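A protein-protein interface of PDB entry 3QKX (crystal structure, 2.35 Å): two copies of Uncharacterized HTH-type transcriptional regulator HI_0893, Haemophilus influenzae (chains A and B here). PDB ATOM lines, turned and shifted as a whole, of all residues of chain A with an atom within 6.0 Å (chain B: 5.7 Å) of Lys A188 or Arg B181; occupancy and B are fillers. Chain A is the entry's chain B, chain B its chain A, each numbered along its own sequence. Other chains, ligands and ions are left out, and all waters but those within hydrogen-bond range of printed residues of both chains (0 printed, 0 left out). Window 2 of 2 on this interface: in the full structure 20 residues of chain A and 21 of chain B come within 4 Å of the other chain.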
ATOM      1  N   GLY A 138     -33.583   1.838 -15.382  1.00  0.00           N
ATOM      2  CA  GLY A 138     -32.283   2.398 -15.000  1.00  0.00           C
ATOM      3  C   GLY A 138     -32.336   3.348 -13.814  1.00  0.00           C
ATOM      4  O   GLY A 138     -31.358   4.043 -13.554  1.00  0.00           O
ATOM      5  N   LEU A 139     -33.449   3.353 -13.072  1.00  0.00           N
ATOM      6  CA  LEU A 139     -33.671   4.341 -11.994  1.00  0.00           C
ATOM      7  C   LEU A 139     -33.125   3.882 -10.630  1.00  0.00           C
ATOM      8  O   LEU A 139     -32.514   4.674  -9.907  1.00  0.00           O
ATOM      9  CB  LEU A 139     -35.167   4.689 -11.847  1.00  0.00           C
ATOM     10  CG  LEU A 139     -35.773   5.735 -12.793  1.00  0.00           C
ATOM     11  CD1 LEU A 139     -35.854   5.205 -14.209  1.00  0.00           C
ATOM     12  CD2 LEU A 139     -37.168   6.175 -12.321  1.00  0.00           C
ATOM     13  N   LEU A 140     -33.357   2.617 -10.280  1.00  0.00           N
ATOM     14  CA  LEU A 140     -33.075   2.120  -8.933  1.00  0.00           C
ATOM     15  C   LEU A 140     -31.742   1.412  -8.850  1.00  0.00           C
ATOM     16  O   LEU A 140     -31.246   0.929  -9.847  1.00  0.00           O
ATOM     17  CB  LEU A 140     -34.166   1.153  -8.481  1.00  0.00           C
ATOM     18  CG  LEU A 140     -35.581   1.701  -8.312  1.00  0.00           C
ATOM     19  CD1 LEU A 140     -36.516   0.643  -7.724  1.00  0.00           C
ATOM     20  CD2 LEU A 140     -35.583   2.928  -7.432  1.00  0.00           C
ATOM     21  N   ALA A 141     -31.186   1.328  -7.638  1.00  0.00           N
ATOM     22  CA  ALA A 141     -29.959   0.548  -7.383  1.00  0.00           C
ATOM     23  C   ALA A 141     -30.193  -0.921  -7.678  1.00  0.00           C
ATOM     24  O   ALA A 141     -31.280  -1.404  -7.472  1.00  0.00           O
ATOM     25  CB  ALA A 141     -29.523   0.719  -5.917  1.00  0.00           C
ATOM     26  N   GLU A 142     -29.181  -1.642  -8.152  1.00  0.00           N
ATOM     27  CA  GLU A 142     -29.291  -3.112  -8.275  1.00  0.00           C
ATOM     28  C   GLU A 142     -28.962  -3.725  -6.913  1.00  0.00           C
ATOM     29  O   GLU A 142     -27.841  -4.166  -6.659  1.00  0.00           O
ATOM     30  CB  GLU A 142     -28.404  -3.671  -9.413  1.00  0.00           C
ATOM     31  CG  GLU A 142     -29.128  -3.767 -10.813  1.00  0.00           C
ATOM     32  N   LEU A 143     -29.935  -3.627  -6.011  1.00  0.00           N
ATOM     33  CA  LEU A 143     -29.920  -4.273  -4.705  1.00  0.00           C
ATOM     34  C   LEU A 143     -31.191  -5.069  -4.645  1.00  0.00           C
ATOM     35  O   LEU A 143     -32.111  -4.789  -5.381  1.00  0.00           O
ATOM     36  CB  LEU A 143     -29.936  -3.250  -3.584  1.00  0.00           C
ATOM     37  CG  LEU A 143     -28.644  -2.510  -3.273  1.00  0.00           C
ATOM     38  CD1 LEU A 143     -28.959  -1.397  -2.300  1.00  0.00           C
ATOM     39  CD2 LEU A 143     -27.599  -3.433  -2.695  1.00  0.00           C
ATOM     40  N   LEU A 151     -34.731   0.545   2.847  1.00  0.00           N
ATOM     41  CA  LEU A 151     -34.117   1.873   2.688  1.00  0.00           C
ATOM     42  C   LEU A 151     -35.188   2.934   2.362  1.00  0.00           C
ATOM     43  O   LEU A 151     -34.976   4.114   2.610  1.00  0.00           O
ATOM     44  CB  LEU A 151     -33.069   1.845   1.583  1.00  0.00           C
ATOM     45  CG  LEU A 151     -31.682   1.274   1.888  1.00  0.00           C
ATOM     46  CD1 LEU A 151     -30.930   0.999   0.617  1.00  0.00           C
ATOM     47  CD2 LEU A 151     -30.905   2.237   2.750  1.00  0.00           C
ATOM     48  N   ARG A 184     -34.533   8.935  -2.650  1.00  0.00           N
ATOM     49  CA  ARG A 184     -33.141   9.264  -2.899  1.00  0.00           C
ATOM     50  C   ARG A 184     -32.199   8.110  -2.507  1.00  0.00           C
ATOM     51  O   ARG A 184     -31.248   7.819  -3.210  1.00  0.00           O
ATOM     52  CB  ARG A 184     -32.772  10.518  -2.112  1.00  0.00           C
ATOM     53  CG  ARG A 184     -31.756  11.321  -2.739  1.00  0.00           C
ATOM     54  CD  ARG A 184     -31.257  12.407  -1.808  1.00  0.00           C
ATOM     55  NE  ARG A 184     -32.226  13.491  -1.569  1.00  0.00           N
ATOM     56  CZ  ARG A 184     -31.909  14.685  -1.032  1.00  0.00           C
ATOM     57  NH1 ARG A 184     -30.651  14.978  -0.670  1.00  0.00           N
ATOM     58  NH2 ARG A 184     -32.854  15.606  -0.861  1.00  0.00           N
ATOM     59  N   ALA A 185     -32.498   7.450  -1.386  1.00  0.00           N
ATOM     60  CA  ALA A 185     -31.671   6.351  -0.871  1.00  0.00           C
ATOM     61  C   ALA A 185     -31.572   5.154  -1.811  1.00  0.00           C
ATOM     62  O   ALA A 185     -30.619   4.405  -1.713  1.00  0.00           O
ATOM     63  CB  ALA A 185     -32.208   5.891   0.476  1.00  0.00           C
ATOM     64  N   ILE A 186     -32.581   4.946  -2.679  1.00  0.00           N
ATOM     65  CA  ILE A 186     -32.592   3.792  -3.591  1.00  0.00           C
ATOM     66  C   ILE A 186     -32.404   4.161  -5.069  1.00  0.00           C
ATOM     67  O   ILE A 186     -32.748   3.385  -5.945  1.00  0.00           O
ATOM     68  CB  ILE A 186     -33.870   2.906  -3.398  1.00  0.00           C
ATOM     69  CG1 ILE A 186     -35.157   3.613  -3.839  1.00  0.00           C
ATOM     70  CG2 ILE A 186     -34.003   2.486  -1.942  1.00  0.00           C
ATOM     71  CD1 ILE A 186     -36.368   2.737  -3.695  1.00  0.00           C
ATOM     72  N   GLN A 187     -31.823   5.327  -5.331  1.00  0.00           N
ATOM     73  CA  GLN A 187     -31.494   5.735  -6.692  1.00  0.00           C
ATOM     74  C   GLN A 187     -30.190   5.095  -7.123  1.00  0.00           C
ATOM     75  O   GLN A 187     -29.252   5.064  -6.335  1.00  0.00           O
ATOM     76  CB  GLN A 187     -31.337   7.253  -6.760  1.00  0.00           C
ATOM     77  CG  GLN A 187     -32.574   8.045  -6.361  1.00  0.00           C
ATOM     78  CD  GLN A 187     -33.725   7.714  -7.224  1.00  0.00           C
ATOM     79  OE1 GLN A 187     -34.598   6.948  -6.820  1.00  0.00           O
ATOM     80  NE2 GLN A 187     -33.700   8.198  -8.475  1.00  0.00           N
ATOM     81  N   LYS A 188     -30.125   4.616  -8.375  1.00  0.00           N
ATOM     82  CA  LYS A 188     -28.904   4.018  -8.942  1.00  0.00           C
ATOM     83  C   LYS A 188     -27.730   4.960  -8.745  1.00  0.00           C
ATOM     84  O   LYS A 188     -26.625   4.552  -8.363  1.00  0.00           O
ATOM     85  CB  LYS A 188     -29.094   3.715 -10.433  1.00  0.00           C
ATOM     86  CG  LYS A 188     -27.886   3.018 -11.136  1.00  0.00           C
ATOM     87  CD  LYS A 188     -28.209   2.639 -12.623  1.00  0.00           C
ATOM     88  CE  LYS A 188     -26.951   2.492 -13.491  1.00  0.00           C
ATOM     89  OXT LYS A 188     -27.895   6.164  -8.923  1.00  0.00           O
ATOM     90  N   GLU B 176     -22.057  -1.915   3.189  1.00  0.00           N
ATOM     91  CA  GLU B 176     -21.545  -0.581   2.881  1.00  0.00           C
ATOM     92  C   GLU B 176     -22.518   0.180   2.004  1.00  0.00           C
ATOM     93  O   GLU B 176     -22.722   1.391   2.189  1.00  0.00           O
ATOM     94  CB  GLU B 176     -20.182  -0.665   2.164  1.00  0.00           C
ATOM     95  CG  GLU B 176     -19.041  -1.321   2.972  1.00  0.00           C
ATOM     96  CD  GLU B 176     -18.603  -0.537   4.192  1.00  0.00           C
ATOM     97  OE1 GLU B 176     -18.990   0.640   4.330  1.00  0.00           O
ATOM     98  OE2 GLU B 176     -17.847  -1.102   5.018  1.00  0.00           O
ATOM     99  N   SER B 177     -23.118  -0.518   1.043  1.00  0.00           N
ATOM    100  CA  SER B 177     -24.183   0.078   0.243  1.00  0.00           C
ATOM    101  C   SER B 177     -25.282   0.637   1.128  1.00  0.00           C
ATOM    102  O   SER B 177     -25.628   1.787   0.987  1.00  0.00           O
ATOM    103  CB  SER B 177     -24.756  -0.917  -0.760  1.00  0.00           C
ATOM    104  OG  SER B 177     -24.015  -0.893  -1.971  1.00  0.00           O
ATOM    105  N   VAL B 178     -25.758  -0.143   2.096  1.00  0.00           N
ATOM    106  CA  VAL B 178     -26.795   0.344   3.025  1.00  0.00           C
ATOM    107  C   VAL B 178     -26.300   1.492   3.906  1.00  0.00           C
ATOM    108  O   VAL B 178     -27.023   2.456   4.133  1.00  0.00           O
ATOM    109  CB  VAL B 178     -27.342  -0.768   3.928  1.00  0.00           C
ATOM    110  CG1 VAL B 178     -28.310  -0.201   4.887  1.00  0.00           C
ATOM    111  CG2 VAL B 178     -27.998  -1.873   3.108  1.00  0.00           C
ATOM    112  N   ILE B 179     -25.066   1.405   4.389  1.00  0.00           N
ATOM    113  CA  ILE B 179     -24.489   2.504   5.171  1.00  0.00           C
ATOM    114  C   ILE B 179     -24.454   3.796   4.359  1.00  0.00           C
ATOM    115  O   ILE B 179     -24.888   4.820   4.815  1.00  0.00           O
ATOM    116  CB  ILE B 179     -23.069   2.210   5.643  1.00  0.00           C
ATOM    117  CG1 ILE B 179     -23.073   1.201   6.771  1.00  0.00           C
ATOM    118  CG2 ILE B 179     -22.408   3.490   6.171  1.00  0.00           C
ATOM    119  CD1 ILE B 179     -21.675   0.557   7.042  1.00  0.00           C
ATOM    120  N   GLU B 180     -23.925   3.716   3.161  1.00  0.00           N
ATOM    121  CA  GLU B 180     -23.778   4.877   2.289  1.00  0.00           C
ATOM    122  C   GLU B 180     -25.105   5.426   1.813  1.00  0.00           C
ATOM    123  O   GLU B 180     -25.276   6.631   1.717  1.00  0.00           O
ATOM    124  CB  GLU B 180     -22.919   4.515   1.081  1.00  0.00           C
ATOM    125  CG  GLU B 180     -22.521   5.728   0.226  1.00  0.00           C
ATOM    126  CD  GLU B 180     -23.512   6.037  -0.889  1.00  0.00           C
ATOM    127  OE1 GLU B 180     -23.913   5.094  -1.625  1.00  0.00           O
ATOM    128  OE2 GLU B 180     -23.888   7.226  -1.039  1.00  0.00           O
ATOM    129  N   ARG B 181     -26.033   4.546   1.491  1.00  0.00           N
ATOM    130  CA  ARG B 181     -27.329   4.971   0.968  1.00  0.00           C
ATOM    131  C   ARG B 181     -28.221   5.531   2.056  1.00  0.00           C
ATOM    132  O   ARG B 181     -28.934   6.501   1.811  1.00  0.00           O
ATOM    133  CB  ARG B 181     -27.996   3.822   0.253  1.00  0.00           C
ATOM    134  CG  ARG B 181     -27.341   3.583  -1.079  1.00  0.00           C
ATOM    135  CD  ARG B 181     -27.875   2.394  -1.770  1.00  0.00           C
ATOM    136  NE  ARG B 181     -27.323   2.275  -3.108  1.00  0.00           N
ATOM    137  CZ  ARG B 181     -27.681   3.015  -4.160  1.00  0.00           C
ATOM    138  NH1 ARG B 181     -28.609   3.974  -4.059  1.00  0.00           N
ATOM    139  NH2 ARG B 181     -27.103   2.799  -5.333  1.00  0.00           N
ATOM    140  N   SER B 182     -28.182   4.950   3.258  1.00  0.00           N
ATOM    141  CA  SER B 182     -28.954   5.517   4.380  1.00  0.00           C
ATOM    142  C   SER B 182     -28.427   6.919   4.773  1.00  0.00           C
ATOM    143  O   SER B 182     -29.204   7.813   5.130  1.00  0.00           O
ATOM    144  CB  SER B 182     -28.909   4.583   5.571  1.00  0.00           C
ATOM    145  OG  SER B 182     -27.593   4.480   6.030  1.00  0.00           O
ATOM    146  N   TRP B 183     -27.102   7.087   4.702  1.00  0.00           N
ATOM    147  CA  TRP B 183     -26.444   8.395   4.852  1.00  0.00           C
ATOM    148  C   TRP B 183     -26.923   9.373   3.812  1.00  0.00           C
ATOM    149  O   TRP B 183     -27.231  10.512   4.123  1.00  0.00           O
ATOM    150  CB  TRP B 183     -24.951   8.218   4.714  1.00  0.00           C
ATOM    151  CG  TRP B 183     -24.127   9.487   4.656  1.00  0.00           C
ATOM    152  CD1 TRP B 183     -23.399   9.927   3.600  1.00  0.00           C
ATOM    153  CD2 TRP B 183     -23.861  10.383   5.721  1.00  0.00           C
ATOM    154  NE1 TRP B 183     -22.727  11.060   3.928  1.00  0.00           N
ATOM    155  CE2 TRP B 183     -22.981  11.359   5.231  1.00  0.00           C
ATOM    156  CE3 TRP B 183     -24.280  10.459   7.042  1.00  0.00           C
ATOM    157  CZ2 TRP B 183     -22.534  12.420   6.005  1.00  0.00           C
ATOM    158  CZ3 TRP B 183     -23.839  11.512   7.815  1.00  0.00           C
ATOM    159  CH2 TRP B 183     -22.977  12.484   7.297  1.00  0.00           C
ATOM    160  N   ARG B 184     -26.999   8.897   2.578  1.00  0.00           N
ATOM    161  CA  ARG B 184     -27.435   9.700   1.439  1.00  0.00           C
ATOM    162  C   ARG B 184     -28.801  10.351   1.697  1.00  0.00           C
ATOM    163  O   ARG B 184     -29.031  11.493   1.322  1.00  0.00           O
ATOM    164  CB  ARG B 184     -27.505   8.825   0.194  1.00  0.00           C
ATOM    165  CG  ARG B 184     -27.420   9.565  -1.071  1.00  0.00           C
ATOM    166  CD  ARG B 184     -27.663   8.671  -2.266  1.00  0.00           C
ATOM    167  NE  ARG B 184     -26.603   7.674  -2.504  1.00  0.00           N
ATOM    168  CZ  ARG B 184     -26.526   6.920  -3.610  1.00  0.00           C
ATOM    169  NH1 ARG B 184     -27.451   7.028  -4.571  1.00  0.00           N
ATOM    170  NH2 ARG B 184     -25.531   6.039  -3.767  1.00  0.00           N
ATOM    171  N   ALA B 185     -29.691   9.611   2.354  1.00  0.00           N
ATOM    172  CA  ALA B 185     -31.030  10.082   2.684  1.00  0.00           C
ATOM    173  C   ALA B 185     -31.073  11.315   3.606  1.00  0.00           C
ATOM    174  O   ALA B 185     -32.067  12.049   3.607  1.00  0.00           O
ATOM    175  CB  ALA B 185     -31.824   8.935   3.320  1.00  0.00           C
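The backbone carbonyl oxygen of Leu A139 is in hydrogen-bond range of the backbone NH of Lys A188 (2.8 Å). The side-chain hydroxyl of Ser B182 is in hydrogen-bond range of the backbone carbonyl oxygen of Val B178, 2.8 Å away. The side-chain carboxylate (OE1) of Glu B180 lies within salt-bridge range of the guanidinium group (NH2) of Arg B184 (2.8 Å). O of Ile B179 is in hydrogen-bond range of OG of Ser B182 (3.0 Å). The backbone carbonyl oxygen (O) of Ile A186 sits at hydrogen-bond distance from the backbone NH (N) of Ala A141, 3.1 Å away.
NH1 of Arg B181 is in hydrogen-bond range of O of Gln A187 (2.6 Å). The guanidinium group (NH1) of Arg B184 sits at hydrogen-bond distance from the backbone carbonyl oxygen (O) of Gln A187. The guanidinium group of Arg B181 is in salt-bridge range of the chain-end carboxylate of Lys A188. The backbone carbonyl oxygen (O) of Ala A185 is in hydrogen-bond range of the guanidinium group (NH1) of Arg B181 (3.1 Å).
Arg B184 touches its own counterpart, Arg A184. Of the 9 pairs that touch across the chains among the printed residues, 1 has its exchanged pair printed and touching as well.
Arg B181 touches just these residues of chain A: Ala A141 (3.2 Å), Leu A143 (3.98 Å), Ala A185 (3.1 Å), Ile A186 (3.9 Å), Gln A187 (2.6 Å) and Lys A188 (3.5 Å). Of the printed residues of chain B, Ile A186 touches Arg B181. Of the printed residues of chain B, Leu A143 touches Arg B181 (3.98 Å). The nearest printed residue of chain B that does not touch Leu A143 is Ser B177 (4.3 Å).
Of the 10 printed residues of chain B, 3 touch a printed residue of chain A. Along chain B the printed residues that touch a printed residue of chain A span positions 181 to 184.
CB of Ala A141 touches NH2 of Arg B181, 3.2 Å away. Leu A143 touches Arg B181. Leu A151 touches Ser B182 (CD2 to N, 3.9 Å). Arg A184 touches Arg B184. C of Ile A186 touches NH1 of Arg B181, at 3.9 Å.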
